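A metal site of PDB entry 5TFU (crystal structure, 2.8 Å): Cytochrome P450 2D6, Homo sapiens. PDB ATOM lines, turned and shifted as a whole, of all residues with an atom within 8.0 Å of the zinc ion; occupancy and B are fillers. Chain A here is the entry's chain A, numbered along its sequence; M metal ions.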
ATOM      1  N   TRP A 130      28.478 -11.139  -6.968  1.00  0.00           N
ATOM      2  CA  TRP A 130      28.821 -11.111  -5.555  1.00  0.00           C
ATOM      3  C   TRP A 130      29.998 -10.177  -5.263  1.00  0.00           C
ATOM      4  O   TRP A 130      30.042  -9.547  -4.215  1.00  0.00           O
ATOM      5  CB  TRP A 130      29.136 -12.521  -5.042  1.00  0.00           C
ATOM      6  CG  TRP A 130      27.922 -13.342  -4.720  1.00  0.00           C
ATOM      7  CD1 TRP A 130      26.835 -12.952  -3.996  1.00  0.00           C
ATOM      8  CD2 TRP A 130      27.676 -14.700  -5.107  1.00  0.00           C
ATOM      9  NE1 TRP A 130      25.922 -13.980  -3.914  1.00  0.00           N
ATOM     10  CE2 TRP A 130      26.415 -15.064  -4.584  1.00  0.00           C
ATOM     11  CE3 TRP A 130      28.397 -15.652  -5.840  1.00  0.00           C
ATOM     12  CZ2 TRP A 130      25.866 -16.332  -4.773  1.00  0.00           C
ATOM     13  CZ3 TRP A 130      27.848 -16.903  -6.031  1.00  0.00           C
ATOM     14  CH2 TRP A 130      26.595 -17.225  -5.498  1.00  0.00           C
ATOM     15  N   ALA A 165      33.108 -16.679   0.784  1.00  0.00           N
ATOM     16  CA  ALA A 165      31.930 -17.208   1.448  1.00  0.00           C
ATOM     17  C   ALA A 165      30.735 -17.253   0.485  1.00  0.00           C
ATOM     18  O   ALA A 165      29.877 -18.115   0.596  1.00  0.00           O
ATOM     19  CB  ALA A 165      31.584 -16.378   2.667  1.00  0.00           C
ATOM     20  N   SER A 166      30.711 -16.317  -0.459  1.00  0.00           N
ATOM     21  CA  SER A 166      29.658 -16.283  -1.462  1.00  0.00           C
ATOM     22  C   SER A 166      29.791 -17.439  -2.447  1.00  0.00           C
ATOM     23  O   SER A 166      28.811 -17.858  -3.051  1.00  0.00           O
ATOM     24  CB  SER A 166      29.686 -14.946  -2.213  1.00  0.00           C
ATOM     25  OG  SER A 166      29.390 -13.860  -1.357  1.00  0.00           O
ATOM     26  N   LEU A 167      31.008 -17.937  -2.614  1.00  0.00           N
ATOM     27  CA  LEU A 167      31.256 -19.035  -3.532  1.00  0.00           C
ATOM     28  C   LEU A 167      31.159 -20.376  -2.820  1.00  0.00           C
ATOM     29  O   LEU A 167      30.690 -21.362  -3.394  1.00  0.00           O
ATOM     30  CB  LEU A 167      32.626 -18.889  -4.199  1.00  0.00           C
ATOM     31  CG  LEU A 167      32.781 -17.638  -5.057  1.00  0.00           C
ATOM     32  CD1 LEU A 167      34.049 -17.702  -5.884  1.00  0.00           C
ATOM     33  CD2 LEU A 167      31.560 -17.440  -5.940  1.00  0.00           C
ATOM     34  N   THR A 168      31.607 -20.417  -1.571  1.00  0.00           N
ATOM     35  CA  THR A 168      31.520 -21.637  -0.779  1.00  0.00           C
ATOM     36  C   THR A 168      30.130 -21.802  -0.177  1.00  0.00           C
ATOM     37  O   THR A 168      29.386 -22.705  -0.556  1.00  0.00           O
ATOM     38  CB  THR A 168      32.555 -21.655   0.349  1.00  0.00           C
ATOM     39  OG1 THR A 168      32.271 -20.612   1.284  1.00  0.00           O
ATOM     40  CG2 THR A 168      33.955 -21.473  -0.210  1.00  0.00           C
ATOM     41  N   CYS A 169      29.783 -20.915   0.761  1.00  0.00           N
ATOM     42  CA  CYS A 169      28.540 -21.041   1.516  1.00  0.00           C
ATOM     43  C   CYS A 169      27.363 -20.290   0.871  1.00  0.00           C
ATOM     44  O   CYS A 169      26.240 -20.377   1.363  1.00  0.00           O
ATOM     45  CB  CYS A 169      28.743 -20.530   2.948  1.00  0.00           C
ATOM     46  SG  CYS A 169      30.182 -21.218   3.816  1.00  0.00           S
ATOM     47  N   GLY A 170      27.624 -19.582  -0.212  1.00  0.00           N
ATOM     48  CA  GLY A 170      26.579 -18.860  -0.921  1.00  0.00           C
ATOM     49  C   GLY A 170      25.982 -17.704  -0.124  1.00  0.00           C
ATOM     50  O   GLY A 170      24.833 -17.329  -0.321  1.00  0.00           O
ATOM     51  N   ARG A 171      26.790 -17.130   0.766  1.00  0.00           N
ATOM     52  CA  ARG A 171      26.330 -16.035   1.612  1.00  0.00           C
ATOM     53  C   ARG A 171      27.456 -15.067   1.943  1.00  0.00           C
ATOM     54  O   ARG A 171      28.630 -15.378   1.767  1.00  0.00           O
ATOM     55  CB  ARG A 171      25.733 -16.575   2.914  1.00  0.00           C
ATOM     56  CG  ARG A 171      26.778 -17.139   3.861  1.00  0.00           C
ATOM     57  CD  ARG A 171      26.273 -17.188   5.286  1.00  0.00           C
ATOM     58  NE  ARG A 171      26.047 -15.863   5.833  1.00  0.00           N
ATOM     59  CZ  ARG A 171      25.554 -15.613   7.041  1.00  0.00           C
ATOM     60  NH1 ARG A 171      25.240 -16.629   7.840  1.00  0.00           N
ATOM     61  NH2 ARG A 171      25.383 -14.376   7.456  1.00  0.00           N
ATOM     62  N   HIS A 236      24.579 -24.373   6.938  1.00  0.00           N
ATOM     63  CA  HIS A 236      24.403 -24.340   5.491  1.00  0.00           C
ATOM     64  C   HIS A 236      23.740 -25.612   4.962  1.00  0.00           C
ATOM     65  O   HIS A 236      22.943 -25.565   4.022  1.00  0.00           O
ATOM     66  CB  HIS A 236      25.744 -24.133   4.798  1.00  0.00           C
ATOM     67  CG  HIS A 236      25.638 -23.936   3.325  1.00  0.00           C
ATOM     68  ND1 HIS A 236      26.623 -24.325   2.442  1.00  0.00           N
ATOM     69  CD2 HIS A 236      24.660 -23.378   2.568  1.00  0.00           C
ATOM     70  CE1 HIS A 236      26.253 -24.028   1.207  1.00  0.00           C
ATOM     71  NE2 HIS A 236      25.073 -23.452   1.261  1.00  0.00           N
ATOM     72  N   ARG A 237      24.067 -26.749   5.572  1.00  0.00           N
ATOM     73  CA  ARG A 237      23.499 -28.026   5.165  1.00  0.00           C
ATOM     74  C   ARG A 237      21.992 -28.047   5.408  1.00  0.00           C
ATOM     75  O   ARG A 237      21.258 -28.745   4.709  1.00  0.00           O
ATOM     76  CB  ARG A 237      24.167 -29.175   5.926  1.00  0.00           C
ATOM     77  CG  ARG A 237      23.864 -30.559   5.362  1.00  0.00           C
ATOM     78  CD  ARG A 237      24.412 -31.652   6.270  1.00  0.00           C
ATOM     79  NE  ARG A 237      25.848 -31.512   6.499  1.00  0.00           N
ATOM     80  CZ  ARG A 237      26.782 -32.198   5.849  1.00  0.00           C
ATOM     81  NH1 ARG A 237      26.426 -33.073   4.924  1.00  0.00           N
ATOM     82  NH2 ARG A 237      28.056 -32.002   6.120  1.00  0.00           N
ATOM     83  N   THR A 239      19.921 -25.380   5.118  1.00  0.00           N
ATOM     84  CA  THR A 239      19.223 -24.508   4.180  1.00  0.00           C
ATOM     85  C   THR A 239      19.361 -24.965   2.732  1.00  0.00           C
ATOM     86  O   THR A 239      18.739 -24.400   1.830  1.00  0.00           O
ATOM     87  CB  THR A 239      19.721 -23.052   4.280  1.00  0.00           C
ATOM     88  OG1 THR A 239      21.132 -23.012   3.986  1.00  0.00           O
ATOM     89  CG2 THR A 239      19.487 -22.505   5.682  1.00  0.00           C
ATOM     90  N   TRP A 240      20.191 -25.973   2.511  1.00  0.00           N
ATOM     91  CA  TRP A 240      20.463 -26.457   1.157  1.00  0.00           C
ATOM     92  C   TRP A 240      19.249 -27.172   0.559  1.00  0.00           C
ATOM     93  O   TRP A 240      18.701 -28.097   1.154  1.00  0.00           O
ATOM     94  CB  TRP A 240      21.678 -27.388   1.161  1.00  0.00           C
ATOM     95  CG  TRP A 240      21.852 -28.177  -0.095  1.00  0.00           C
ATOM     96  CD1 TRP A 240      21.827 -27.707  -1.376  1.00  0.00           C
ATOM     97  CD2 TRP A 240      22.100 -29.586  -0.189  1.00  0.00           C
ATOM     98  NE1 TRP A 240      22.034 -28.730  -2.259  1.00  0.00           N
ATOM     99  CE2 TRP A 240      22.203 -29.893  -1.561  1.00  0.00           C
ATOM    100  CE3 TRP A 240      22.237 -30.613   0.746  1.00  0.00           C
ATOM    101  CZ2 TRP A 240      22.443 -31.190  -2.023  1.00  0.00           C
ATOM    102  CZ3 TRP A 240      22.480 -31.898   0.290  1.00  0.00           C
ATOM    103  CH2 TRP A 240      22.570 -32.170  -1.080  1.00  0.00           C
ATOM    104  N   ASP A 241      18.843 -26.722  -0.622  1.00  0.00           N
ATOM    105  CA  ASP A 241      17.748 -27.352  -1.359  1.00  0.00           C
ATOM    106  C   ASP A 241      18.293 -28.174  -2.523  1.00  0.00           C
ATOM    107  O   ASP A 241      18.690 -27.612  -3.546  1.00  0.00           O
ATOM    108  CB  ASP A 241      16.758 -26.302  -1.857  1.00  0.00           C
ATOM    109  CG  ASP A 241      15.485 -26.917  -2.413  1.00  0.00           C
ATOM    110  OD1 ASP A 241      14.726 -26.206  -3.108  1.00  0.00           O
ATOM    111  OD2 ASP A 241      15.239 -28.113  -2.157  1.00  0.00           O
ATOM    112  N   PRO A 245      19.401 -26.594  -8.637  1.00  0.00           N
ATOM    113  CA  PRO A 245      20.830 -26.612  -8.972  1.00  0.00           C
ATOM    114  C   PRO A 245      21.649 -25.888  -7.912  1.00  0.00           C
ATOM    115  O   PRO A 245      21.186 -24.870  -7.402  1.00  0.00           O
ATOM    116  CB  PRO A 245      20.890 -25.890 -10.315  1.00  0.00           C
ATOM    117  CG  PRO A 245      19.533 -26.064 -10.896  1.00  0.00           C
ATOM    118  CD  PRO A 245      18.587 -26.036  -9.731  1.00  0.00           C
ATOM    119  N   PRO A 246      22.840 -26.405  -7.583  1.00  0.00           N
ATOM    120  CA  PRO A 246      23.696 -25.840  -6.533  1.00  0.00           C
ATOM    121  C   PRO A 246      23.949 -24.344  -6.711  1.00  0.00           C
ATOM    122  O   PRO A 246      24.385 -23.923  -7.783  1.00  0.00           O
ATOM    123  CB  PRO A 246      24.996 -26.639  -6.664  1.00  0.00           C
ATOM    124  CG  PRO A 246      24.579 -27.926  -7.264  1.00  0.00           C
ATOM    125  CD  PRO A 246      23.453 -27.596  -8.200  1.00  0.00           C
ATOM    126  N   ARG A 247      23.662 -23.568  -5.677  1.00  0.00           N
ATOM    127  CA  ARG A 247      23.923 -22.129  -5.709  1.00  0.00           C
ATOM    128  C   ARG A 247      25.393 -21.827  -5.482  1.00  0.00           C
ATOM    129  O   ARG A 247      25.888 -20.770  -5.871  1.00  0.00           O
ATOM    130  CB  ARG A 247      23.100 -21.390  -4.654  1.00  0.00           C
ATOM    131  CG  ARG A 247      21.625 -21.255  -4.974  1.00  0.00           C
ATOM    132  CD  ARG A 247      21.027 -20.079  -4.201  1.00  0.00           C
ATOM    133  NE  ARG A 247      21.771 -19.770  -2.984  1.00  0.00           N
ATOM    134  CZ  ARG A 247      22.516 -18.678  -2.809  1.00  0.00           C
ATOM    135  NH1 ARG A 247      22.606 -17.783  -3.782  1.00  0.00           N
ATOM    136  NH2 ARG A 247      23.161 -18.487  -1.662  1.00  0.00           N
ATOM    137  N   ASP A 248      26.097 -22.754  -4.846  1.00  0.00           N
ATOM    138  CA  ASP A 248      27.479 -22.533  -4.441  1.00  0.00           C
ATOM    139  C   ASP A 248      28.297 -23.822  -4.447  1.00  0.00           C
ATOM    140  O   ASP A 248      27.764 -24.898  -4.687  1.00  0.00           O
ATOM    141  CB  ASP A 248      27.513 -21.878  -3.058  1.00  0.00           C
ATOM    142  CG  ASP A 248      26.621 -22.583  -2.065  1.00  0.00           C
ATOM    143  OD1 ASP A 248      26.963 -23.709  -1.649  1.00  0.00           O
ATOM    144  OD2 ASP A 248      25.577 -22.016  -1.688  1.00  0.00           O
ATOM    145  N   LEU A 249      29.591 -23.691  -4.173  1.00  0.00           N
ATOM    146  CA  LEU A 249      30.520 -24.800  -4.259  1.00  0.00           C
ATOM    147  C   LEU A 249      30.212 -25.894  -3.241  1.00  0.00           C
ATOM    148  O   LEU A 249      30.356 -27.085  -3.521  1.00  0.00           O
ATOM    149  CB  LEU A 249      31.960 -24.310  -4.067  1.00  0.00           C
ATOM    150  CG  LEU A 249      33.094 -25.324  -4.230  1.00  0.00           C
ATOM    151  CD1 LEU A 249      34.253 -24.688  -4.982  1.00  0.00           C
ATOM    152  CD2 LEU A 249      33.566 -25.829  -2.874  1.00  0.00           C
ATOM    153  N   THR A 250      29.785 -25.491  -2.050  1.00  0.00           N
ATOM    154  CA  THR A 250      29.458 -26.439  -0.989  1.00  0.00           C
ATOM    155  C   THR A 250      28.253 -27.286  -1.389  1.00  0.00           C
ATOM    156  O   THR A 250      28.255 -28.502  -1.197  1.00  0.00           O
ATOM    157  CB  THR A 250      29.173 -25.724   0.348  1.00  0.00           C
ATOM    158  OG1 THR A 250      30.344 -25.002   0.760  1.00  0.00           O
ATOM    159  CG2 THR A 250      28.790 -26.715   1.428  1.00  0.00           C
ATOM    160  N   GLU A 251      27.241 -26.641  -1.961  1.00  0.00           N
ATOM    161  CA  GLU A 251      26.065 -27.349  -2.448  1.00  0.00           C
ATOM    162  C   GLU A 251      26.436 -28.311  -3.560  1.00  0.00           C
ATOM    163  O   GLU A 251      25.871 -29.405  -3.666  1.00  0.00           O
ATOM    164  CB  GLU A 251      24.996 -26.364  -2.920  1.00  0.00           C
ATOM    165  CG  GLU A 251      24.401 -25.518  -1.809  1.00  0.00           C
ATOM    166  CD  GLU A 251      23.301 -24.592  -2.293  1.00  0.00           C
ATOM    167  OE1 GLU A 251      22.800 -24.785  -3.419  1.00  0.00           O
ATOM    168  OE2 GLU A 251      22.935 -23.663  -1.542  1.00  0.00           O
ATOM    169  N   ALA A 252      27.391 -27.903  -4.399  1.00  0.00           N
ATOM    170  CA  ALA A 252      27.885 -28.764  -5.471  1.00  0.00           C
ATOM    171  C   ALA A 252      28.681 -29.927  -4.885  1.00  0.00           C
ATOM    172  O   ALA A 252      28.671 -31.031  -5.436  1.00  0.00           O
ATOM    173  CB  ALA A 252      28.745 -27.962  -6.431  1.00  0.00           C
ATOM    174  N   LEU A 254      28.145 -31.169  -1.786  1.00  0.00           N
ATOM    175  CA  LEU A 254      27.146 -31.992  -1.116  1.00  0.00           C
ATOM    176  C   LEU A 254      26.411 -32.896  -2.105  1.00  0.00           C
ATOM    177  O   LEU A 254      26.115 -34.057  -1.812  1.00  0.00           O
ATOM    178  CB  LEU A 254      26.136 -31.118  -0.364  1.00  0.00           C
ATOM    179  CG  LEU A 254      26.640 -30.300   0.827  1.00  0.00           C
ATOM    180  CD1 LEU A 254      25.556 -29.351   1.322  1.00  0.00           C
ATOM    181  CD2 LEU A 254      27.108 -31.206   1.960  1.00  0.00           C
HETATM  182 ZN    ZN M   1      24.227 -22.735  -0.384  1.00  0.00          ZN
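Cys 169 touches the zinc ion.
Of the 22 residues printed, 4 come within 4 Å of the zinc ion.
The backbone NH of Arg 247 is in hydrogen-bond range of the side-chain carboxylate of Glu 251.
A ring nitrogen (NE2) of His 236 lies close to the backbone carbonyl oxygen (O) of Cys 169.
The backbone carbonyl oxygen (O) of His 236 sits at hydrogen-bond distance from the side-chain hydroxyl (OG1) of Thr 239 (3.1 Å).
OD1 of Asp 248 sits close to N of Thr 250, 3.4 Å away.
The side-chain sulfur (SG) of Cys 169 is in hydrogen-bond range of the side-chain hydroxyl (OG1) of Thr 168.
The zinc ion is bound by OE2 of Glu 251 (2.0 Å), NE2 of His 236 (2.0 Å) and OD2 of Asp 248 (2.0 Å).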
